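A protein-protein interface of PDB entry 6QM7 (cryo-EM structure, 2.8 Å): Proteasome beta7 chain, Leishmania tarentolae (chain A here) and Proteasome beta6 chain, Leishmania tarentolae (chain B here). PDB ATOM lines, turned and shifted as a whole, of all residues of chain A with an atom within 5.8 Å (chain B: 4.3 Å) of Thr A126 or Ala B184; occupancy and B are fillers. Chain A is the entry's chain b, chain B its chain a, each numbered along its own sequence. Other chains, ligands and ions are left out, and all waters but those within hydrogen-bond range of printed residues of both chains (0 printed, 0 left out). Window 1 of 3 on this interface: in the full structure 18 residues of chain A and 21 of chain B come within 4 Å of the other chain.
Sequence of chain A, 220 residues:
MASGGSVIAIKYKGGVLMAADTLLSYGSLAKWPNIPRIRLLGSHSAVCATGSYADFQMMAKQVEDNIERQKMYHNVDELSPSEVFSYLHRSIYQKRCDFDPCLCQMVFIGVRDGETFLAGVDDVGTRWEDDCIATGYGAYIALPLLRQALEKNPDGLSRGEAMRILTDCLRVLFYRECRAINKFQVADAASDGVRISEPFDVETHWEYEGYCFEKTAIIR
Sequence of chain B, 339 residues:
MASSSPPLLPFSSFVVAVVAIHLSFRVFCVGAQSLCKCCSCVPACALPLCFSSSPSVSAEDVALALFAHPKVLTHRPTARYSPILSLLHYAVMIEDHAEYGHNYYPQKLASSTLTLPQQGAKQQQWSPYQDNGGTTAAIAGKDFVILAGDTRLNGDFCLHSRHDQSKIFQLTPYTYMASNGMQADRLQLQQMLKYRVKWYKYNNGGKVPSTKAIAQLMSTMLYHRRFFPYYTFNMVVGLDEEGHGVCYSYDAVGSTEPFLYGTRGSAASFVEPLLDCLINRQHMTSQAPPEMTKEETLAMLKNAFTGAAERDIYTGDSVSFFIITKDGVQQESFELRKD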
ATOM      1  N   HIS A  89     -17.702   9.616 -18.804  1.00  0.00           N
ATOM      2  CA  HIS A  89     -18.746   8.578 -18.925  1.00  0.00           C
ATOM      3  C   HIS A  89     -20.048   9.085 -18.297  1.00  0.00           C
ATOM      4  O   HIS A  89     -21.104   8.979 -18.947  1.00  0.00           O
ATOM      5  CB  HIS A  89     -18.276   7.258 -18.308  1.00  0.00           C
ATOM      6  CG  HIS A  89     -19.423   6.362 -18.018  1.00  0.00           C
ATOM      7  ND1 HIS A  89     -19.639   5.825 -16.766  1.00  0.00           N
ATOM      8  CD2 HIS A  89     -20.458   5.975 -18.791  1.00  0.00           C
ATOM      9  CE1 HIS A  89     -20.748   5.115 -16.791  1.00  0.00           C
ATOM     10  NE2 HIS A  89     -21.275   5.205 -18.014  1.00  0.00           N
ATOM     11  N   TYR A  93     -23.554   9.945 -20.251  1.00  0.00           N
ATOM     12  CA  TYR A  93     -24.775   9.218 -19.827  1.00  0.00           C
ATOM     13  C   TYR A  93     -25.833  10.213 -19.364  1.00  0.00           C
ATOM     14  O   TYR A  93     -26.999   9.954 -19.626  1.00  0.00           O
ATOM     15  CB  TYR A  93     -24.513   8.234 -18.687  1.00  0.00           C
ATOM     16  CG  TYR A  93     -25.747   7.505 -18.226  1.00  0.00           C
ATOM     17  CD1 TYR A  93     -26.282   6.459 -18.963  1.00  0.00           C
ATOM     18  CD2 TYR A  93     -26.412   7.889 -17.078  1.00  0.00           C
ATOM     19  CE1 TYR A  93     -27.442   5.812 -18.571  1.00  0.00           C
ATOM     20  CE2 TYR A  93     -27.554   7.231 -16.648  1.00  0.00           C
ATOM     21  CZ  TYR A  93     -28.071   6.189 -17.394  1.00  0.00           C
ATOM     22  OH  TYR A  93     -29.213   5.566 -16.967  1.00  0.00           O
ATOM     23  N   GLY A 120     -13.279   2.897 -23.887  1.00  0.00           N
ATOM     24  CA  GLY A 120     -14.205   3.523 -24.835  1.00  0.00           C
ATOM     25  C   GLY A 120     -15.491   3.854 -24.151  1.00  0.00           C
ATOM     26  O   GLY A 120     -15.747   3.263 -23.113  1.00  0.00           O
ATOM     27  N   VAL A 121     -16.260   4.762 -24.733  1.00  0.00           N
ATOM     28  CA  VAL A 121     -17.582   5.185 -24.208  1.00  0.00           C
ATOM     29  C   VAL A 121     -18.464   5.565 -25.385  1.00  0.00           C
ATOM     30  O   VAL A 121     -17.996   6.288 -26.220  1.00  0.00           O
ATOM     31  CB  VAL A 121     -17.434   6.315 -23.179  1.00  0.00           C
ATOM     32  CG1 VAL A 121     -16.761   7.543 -23.751  1.00  0.00           C
ATOM     33  CG2 VAL A 121     -18.763   6.691 -22.542  1.00  0.00           C
ATOM     34  N   ASP A 122     -19.679   5.030 -25.440  1.00  0.00           N
ATOM     35  CA  ASP A 122     -20.681   5.240 -26.515  1.00  0.00           C
ATOM     36  C   ASP A 122     -21.543   6.454 -26.186  1.00  0.00           C
ATOM     37  O   ASP A 122     -21.606   6.842 -25.023  1.00  0.00           O
ATOM     38  CB  ASP A 122     -21.659   4.068 -26.622  1.00  0.00           C
ATOM     39  CG  ASP A 122     -21.283   2.972 -27.605  1.00  0.00           C
ATOM     40  OD1 ASP A 122     -20.171   3.040 -28.191  1.00  0.00           O
ATOM     41  OD2 ASP A 122     -22.116   2.041 -27.778  1.00  0.00           O
ATOM     42  N   ASP A 123     -22.226   6.978 -27.196  1.00  0.00           N
ATOM     43  CA  ASP A 123     -23.333   7.968 -27.114  1.00  0.00           C
ATOM     44  C   ASP A 123     -24.242   7.718 -25.902  1.00  0.00           C
ATOM     45  O   ASP A 123     -24.648   8.722 -25.267  1.00  0.00           O
ATOM     46  CB  ASP A 123     -24.166   7.960 -28.405  1.00  0.00           C
ATOM     47  CG  ASP A 123     -24.308   6.593 -29.082  1.00  0.00           C
ATOM     48  OD1 ASP A 123     -25.446   6.066 -29.127  1.00  0.00           O
ATOM     49  OD2 ASP A 123     -23.267   6.064 -29.586  1.00  0.00           O
ATOM     50  N   VAL A 124     -24.595   6.457 -25.624  1.00  0.00           N
ATOM     51  CA  VAL A 124     -25.619   6.070 -24.606  1.00  0.00           C
ATOM     52  C   VAL A 124     -24.987   5.816 -23.236  1.00  0.00           C
ATOM     53  O   VAL A 124     -25.744   5.516 -22.305  1.00  0.00           O
ATOM     54  CB  VAL A 124     -26.431   4.837 -25.038  1.00  0.00           C
ATOM     55  CG1 VAL A 124     -27.272   5.132 -26.264  1.00  0.00           C
ATOM     56  CG2 VAL A 124     -25.559   3.609 -25.263  1.00  0.00           C
ATOM     57  N   GLY A 125     -23.666   5.903 -23.108  1.00  0.00           N
ATOM     58  CA  GLY A 125     -22.977   5.776 -21.812  1.00  0.00           C
ATOM     59  C   GLY A 125     -22.502   4.364 -21.562  1.00  0.00           C
ATOM     60  O   GLY A 125     -22.165   4.051 -20.411  1.00  0.00           O
ATOM     61  N   THR A 126     -22.474   3.529 -22.602  1.00  0.00           N
ATOM     62  CA  THR A 126     -21.784   2.216 -22.552  1.00  0.00           C
ATOM     63  C   THR A 126     -20.308   2.520 -22.351  1.00  0.00           C
ATOM     64  O   THR A 126     -19.844   3.452 -22.988  1.00  0.00           O
ATOM     65  CB  THR A 126     -21.993   1.386 -23.813  1.00  0.00           C
ATOM     66  OG1 THR A 126     -23.389   1.318 -24.095  1.00  0.00           O
ATOM     67  CG2 THR A 126     -21.431  -0.004 -23.636  1.00  0.00           C
ATOM     68  N   ARG A 127     -19.630   1.838 -21.442  1.00  0.00           N
ATOM     69  CA  ARG A 127     -18.178   2.051 -21.235  1.00  0.00           C
ATOM     70  C   ARG A 127     -17.507   0.697 -21.078  1.00  0.00           C
ATOM     71  O   ARG A 127     -18.139  -0.210 -20.537  1.00  0.00           O
ATOM     72  CB  ARG A 127     -17.907   2.968 -20.041  1.00  0.00           C
ATOM     73  CG  ARG A 127     -18.354   2.429 -18.692  1.00  0.00           C
ATOM     74  CD  ARG A 127     -17.675   3.188 -17.586  1.00  0.00           C
ATOM     75  NE  ARG A 127     -16.331   2.696 -17.295  1.00  0.00           N
ATOM     76  CZ  ARG A 127     -15.481   3.269 -16.438  1.00  0.00           C
ATOM     77  NH1 ARG A 127     -15.822   4.366 -15.780  1.00  0.00           N
ATOM     78  NH2 ARG A 127     -14.279   2.748 -16.246  1.00  0.00           N
ATOM     79  N   TRP A 128     -16.280   0.584 -21.554  1.00  0.00           N
ATOM     80  CA  TRP A 128     -15.526  -0.684 -21.504  1.00  0.00           C
ATOM     81  C   TRP A 128     -14.037  -0.374 -21.539  1.00  0.00           C
ATOM     82  O   TRP A 128     -13.635   0.453 -22.342  1.00  0.00           O
ATOM     83  CB  TRP A 128     -15.969  -1.622 -22.628  1.00  0.00           C
ATOM     84  CG  TRP A 128     -15.677  -1.128 -24.005  1.00  0.00           C
ATOM     85  CD1 TRP A 128     -14.614  -1.478 -24.774  1.00  0.00           C
ATOM     86  CD2 TRP A 128     -16.450  -0.210 -24.793  1.00  0.00           C
ATOM     87  NE1 TRP A 128     -14.649  -0.812 -25.965  1.00  0.00           N
ATOM     88  CE2 TRP A 128     -15.759  -0.025 -26.004  1.00  0.00           C
ATOM     89  CE3 TRP A 128     -17.642   0.493 -24.590  1.00  0.00           C
ATOM     90  CZ2 TRP A 128     -16.217   0.821 -27.010  1.00  0.00           C
ATOM     91  CZ3 TRP A 128     -18.103   1.330 -25.587  1.00  0.00           C
ATOM     92  CH2 TRP A 128     -17.401   1.483 -26.786  1.00  0.00           C
ATOM     93  N   GLN B 130     -29.808   0.337 -25.914  1.00  0.00           N
ATOM     94  CA  GLN B 130     -28.881  -0.587 -26.611  1.00  0.00           C
ATOM     95  C   GLN B 130     -28.870  -1.863 -25.768  1.00  0.00           C
ATOM     96  O   GLN B 130     -28.712  -1.721 -24.558  1.00  0.00           O
ATOM     97  CB  GLN B 130     -27.504   0.078 -26.719  1.00  0.00           C
ATOM     98  CG  GLN B 130     -26.398  -0.804 -27.284  1.00  0.00           C
ATOM     99  CD  GLN B 130     -25.130  -0.040 -27.608  1.00  0.00           C
ATOM    100  OE1 GLN B 130     -24.034  -0.376 -27.148  1.00  0.00           O
ATOM    101  NE2 GLN B 130     -25.263   1.001 -28.418  1.00  0.00           N
ATOM    102  N   ASN B 132     -26.825  -4.906 -24.647  1.00  0.00           N
ATOM    103  CA  ASN B 132     -25.386  -5.247 -24.586  1.00  0.00           C
ATOM    104  C   ASN B 132     -25.246  -6.739 -24.279  1.00  0.00           C
ATOM    105  O   ASN B 132     -24.128  -7.180 -23.945  1.00  0.00           O
ATOM    106  CB  ASN B 132     -24.695  -4.318 -23.593  1.00  0.00           C
ATOM    107  CG  ASN B 132     -24.545  -2.915 -24.135  1.00  0.00           C
ATOM    108  OD1 ASN B 132     -25.168  -1.977 -23.643  1.00  0.00           O
ATOM    109  ND2 ASN B 132     -23.716  -2.763 -25.154  1.00  0.00           N
ATOM    110  N   HIS B 160     -17.473  -5.514 -27.734  1.00  0.00           N
ATOM    111  CA  HIS B 160     -16.681  -4.436 -27.096  1.00  0.00           C
ATOM    112  C   HIS B 160     -15.583  -5.046 -26.230  1.00  0.00           C
ATOM    113  O   HIS B 160     -14.420  -4.613 -26.344  1.00  0.00           O
ATOM    114  CB  HIS B 160     -17.581  -3.547 -26.226  1.00  0.00           C
ATOM    115  CG  HIS B 160     -18.495  -2.651 -26.994  1.00  0.00           C
ATOM    116  ND1 HIS B 160     -18.159  -2.137 -28.234  1.00  0.00           N
ATOM    117  CD2 HIS B 160     -19.698  -2.124 -26.668  1.00  0.00           C
ATOM    118  CE1 HIS B 160     -19.144  -1.366 -28.652  1.00  0.00           C
ATOM    119  NE2 HIS B 160     -20.096  -1.332 -27.705  1.00  0.00           N
ATOM    120  N   MET B 182     -29.108  -3.362 -21.060  1.00  0.00           N
ATOM    121  CA  MET B 182     -28.225  -2.244 -21.438  1.00  0.00           C
ATOM    122  C   MET B 182     -27.200  -2.041 -20.338  1.00  0.00           C
ATOM    123  O   MET B 182     -27.617  -1.949 -19.185  1.00  0.00           O
ATOM    124  CB  MET B 182     -29.025  -0.952 -21.587  1.00  0.00           C
ATOM    125  CG  MET B 182     -28.148   0.209 -21.887  1.00  0.00           C
ATOM    126  SD  MET B 182     -28.869   1.341 -23.042  1.00  0.00           S
ATOM    127  CE  MET B 182     -28.804   2.838 -22.064  1.00  0.00           C
ATOM    128  N   GLN B 183     -25.922  -1.970 -20.704  1.00  0.00           N
ATOM    129  CA  GLN B 183     -24.818  -1.837 -19.733  1.00  0.00           C
ATOM    130  C   GLN B 183     -24.957  -0.494 -19.025  1.00  0.00           C
ATOM    131  O   GLN B 183     -25.012  -0.487 -17.786  1.00  0.00           O
ATOM    132  CB  GLN B 183     -23.447  -1.932 -20.393  1.00  0.00           C
ATOM    133  CG  GLN B 183     -22.338  -2.120 -19.369  1.00  0.00           C
ATOM    134  CD  GLN B 183     -21.126  -1.266 -19.601  1.00  0.00           C
ATOM    135  OE1 GLN B 183     -21.231  -0.094 -19.925  1.00  0.00           O
ATOM    136  NE2 GLN B 183     -19.962  -1.857 -19.399  1.00  0.00           N
ATOM    137  N   ALA B 184     -25.026   0.585 -19.797  1.00  0.00           N
ATOM    138  CA  ALA B 184     -25.040   1.985 -19.317  1.00  0.00           C
ATOM    139  C   ALA B 184     -26.050   2.168 -18.188  1.00  0.00           C
ATOM    140  O   ALA B 184     -25.738   2.925 -17.242  1.00  0.00           O
ATOM    141  CB  ALA B 184     -25.365   2.897 -20.454  1.00  0.00           C
ATOM    142  N   ASP B 185     -27.206   1.514 -18.301  1.00  0.00           N
ATOM    143  CA  ASP B 185     -28.310   1.596 -17.314  1.00  0.00           C
ATOM    144  C   ASP B 185     -27.982   0.729 -16.109  1.00  0.00           C
ATOM    145  O   ASP B 185     -28.226   1.154 -14.984  1.00  0.00           O
ATOM    146  CB  ASP B 185     -29.638   1.188 -17.946  1.00  0.00           C
ATOM    147  CG  ASP B 185     -30.302   2.342 -18.675  1.00  0.00           C
ATOM    148  OD1 ASP B 185     -29.705   3.435 -18.696  1.00  0.00           O
ATOM    149  OD2 ASP B 185     -31.423   2.146 -19.197  1.00  0.00           O
ATOM    150  N   ARG B 186     -27.474  -0.459 -16.348  1.00  0.00           N
ATOM    151  CA  ARG B 186     -27.006  -1.359 -15.270  1.00  0.00           C
ATOM    152  C   ARG B 186     -26.035  -0.553 -14.417  1.00  0.00           C
ATOM    153  O   ARG B 186     -26.204  -0.562 -13.197  1.00  0.00           O
ATOM    154  CB  ARG B 186     -26.477  -2.645 -15.911  1.00  0.00           C
ATOM    155  CG  ARG B 186     -25.288  -3.310 -15.238  1.00  0.00           C
ATOM    156  CD  ARG B 186     -24.430  -4.085 -16.229  1.00  0.00           C
ATOM    157  NE  ARG B 186     -25.152  -4.665 -17.343  1.00  0.00           N
ATOM    158  CZ  ARG B 186     -24.577  -5.277 -18.362  1.00  0.00           C
ATOM    159  NH1 ARG B 186     -23.259  -5.406 -18.407  1.00  0.00           N
ATOM    160  NH2 ARG B 186     -25.325  -5.768 -19.343  1.00  0.00           N
ATOM    161  N   LEU B 187     -25.109   0.177 -15.044  1.00  0.00           N
ATOM    162  CA  LEU B 187     -24.082   0.983 -14.330  1.00  0.00           C
ATOM    163  C   LEU B 187     -24.729   2.123 -13.559  1.00  0.00           C
ATOM    164  O   LEU B 187     -24.237   2.420 -12.495  1.00  0.00           O
ATOM    165  CB  LEU B 187     -23.074   1.562 -15.314  1.00  0.00           C
ATOM    166  CG  LEU B 187     -22.092   0.569 -15.914  1.00  0.00           C
ATOM    167  CD1 LEU B 187     -21.019   1.330 -16.680  1.00  0.00           C
ATOM    168  CD2 LEU B 187     -21.452  -0.316 -14.855  1.00  0.00           C
ATOM    169  N   GLN B 188     -25.738   2.778 -14.109  1.00  0.00           N
ATOM    170  CA  GLN B 188     -26.431   3.878 -13.400  1.00  0.00           C
ATOM    171  C   GLN B 188     -27.180   3.282 -12.209  1.00  0.00           C
ATOM    172  O   GLN B 188     -26.965   3.748 -11.078  1.00  0.00           O
ATOM    173  CB  GLN B 188     -27.407   4.631 -14.302  1.00  0.00           C
ATOM    174  CG  GLN B 188     -28.103   5.788 -13.599  1.00  0.00           C
ATOM    175  CD  GLN B 188     -27.182   6.920 -13.198  1.00  0.00           C
ATOM    176  OE1 GLN B 188     -27.580   7.827 -12.471  1.00  0.00           O
ATOM    177  NE2 GLN B 188     -25.946   6.894 -13.681  1.00  0.00           N
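The side-chain carboxylate of Asp A122 lies close to the side-chain amide oxygen of Gln B130 (3.1 Å).
The side-chain amide nitrogen of Gln B183 sits at hydrogen-bond distance from the backbone carbonyl oxygen of Arg A127 (2.7 Å).
The side-chain carboxylate of Asp B185 sits at hydrogen-bond distance from the side-chain hydroxyl of Tyr A93.
The side-chain amide nitrogen of Asn B132 is in hydrogen-bond range of the side-chain amide oxygen of Gln B130 (3.1 Å).
The backbone NH of Gln B130 lies within hydrogen-bond range of the side-chain sulfur of Met B182, 3.2 Å away.
The side-chain amide oxygen (OD1) of Asn B132 lies within hydrogen-bond range of the backbone NH (N) of Gln B183, at 3.0 Å.
The backbone carbonyl oxygen of Gly A125 lies within hydrogen-bond range of a ring nitrogen (NE2) of His A89.
The backbone carbonyl oxygen (O) of Trp A128 sits at hydrogen-bond distance from the backbone NH (N) of Gly A120 (2.9 Å).
Among the printed residues, pairs that only touch across the chains: His A89 with Leu B187 (3.8 Å), Tyr A93 with Ala B184 (3.6 Å), Tyr A93 with Gln B188 (3.4 Å), Asp A122 with His B160 (3.9 Å), Val A124 with Ala B184 (3.2 Å), Gly A125 with Ala B184 (3.4 Å), Thr A126 with Gln B130 (3.6 Å), Thr A126 with Asn B132 (3.8 Å), Thr A126 with Gln B183 (3.5 Å), Thr A126 with Ala B184 (3.7 Å), Arg A127 with Leu B187 (3.5 Å) and Trp A128 with His B160 (3.5 Å).
Of chain A, only Tyr A93 (3.6 Å), Val A124 (3.2 Å), Gly A125 (3.4 Å) and Thr A126 (3.7 Å) come within 4 Å of Ala B184.
Printed residues of chain A within 4 Å of Gln B130: Asp A122 (3.1 Å) and Thr A126 (3.6 Å).
Printed residues of chain B within 4 Å of Asp A122: Gln B130 (3.1 Å) and His B160 (3.9 Å).
Gly A120 touches none of the printed residues of chain B.
Asp A123 touches none of the printed residues of chain B.
The nearest printed residue of chain B that does not touch Gly A125 is Gln B183 (4.3 Å).
Of the 11 printed residues of chain A, 8 touch a printed residue of chain B.
Hydrophobic or aromatic side chains of chain A that line the printed part of chain B: His A89, Tyr A93 and Trp A128.
Along chain A the printed residues that touch a printed residue of chain B span positions 89 to 128.
Hydrophobic or aromatic side chains of chain B within 4 Å of the printed part of chain A: His B160, Ala B184 and Leu B187.
Among the printed residues, 15 pairs touch across the chains.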
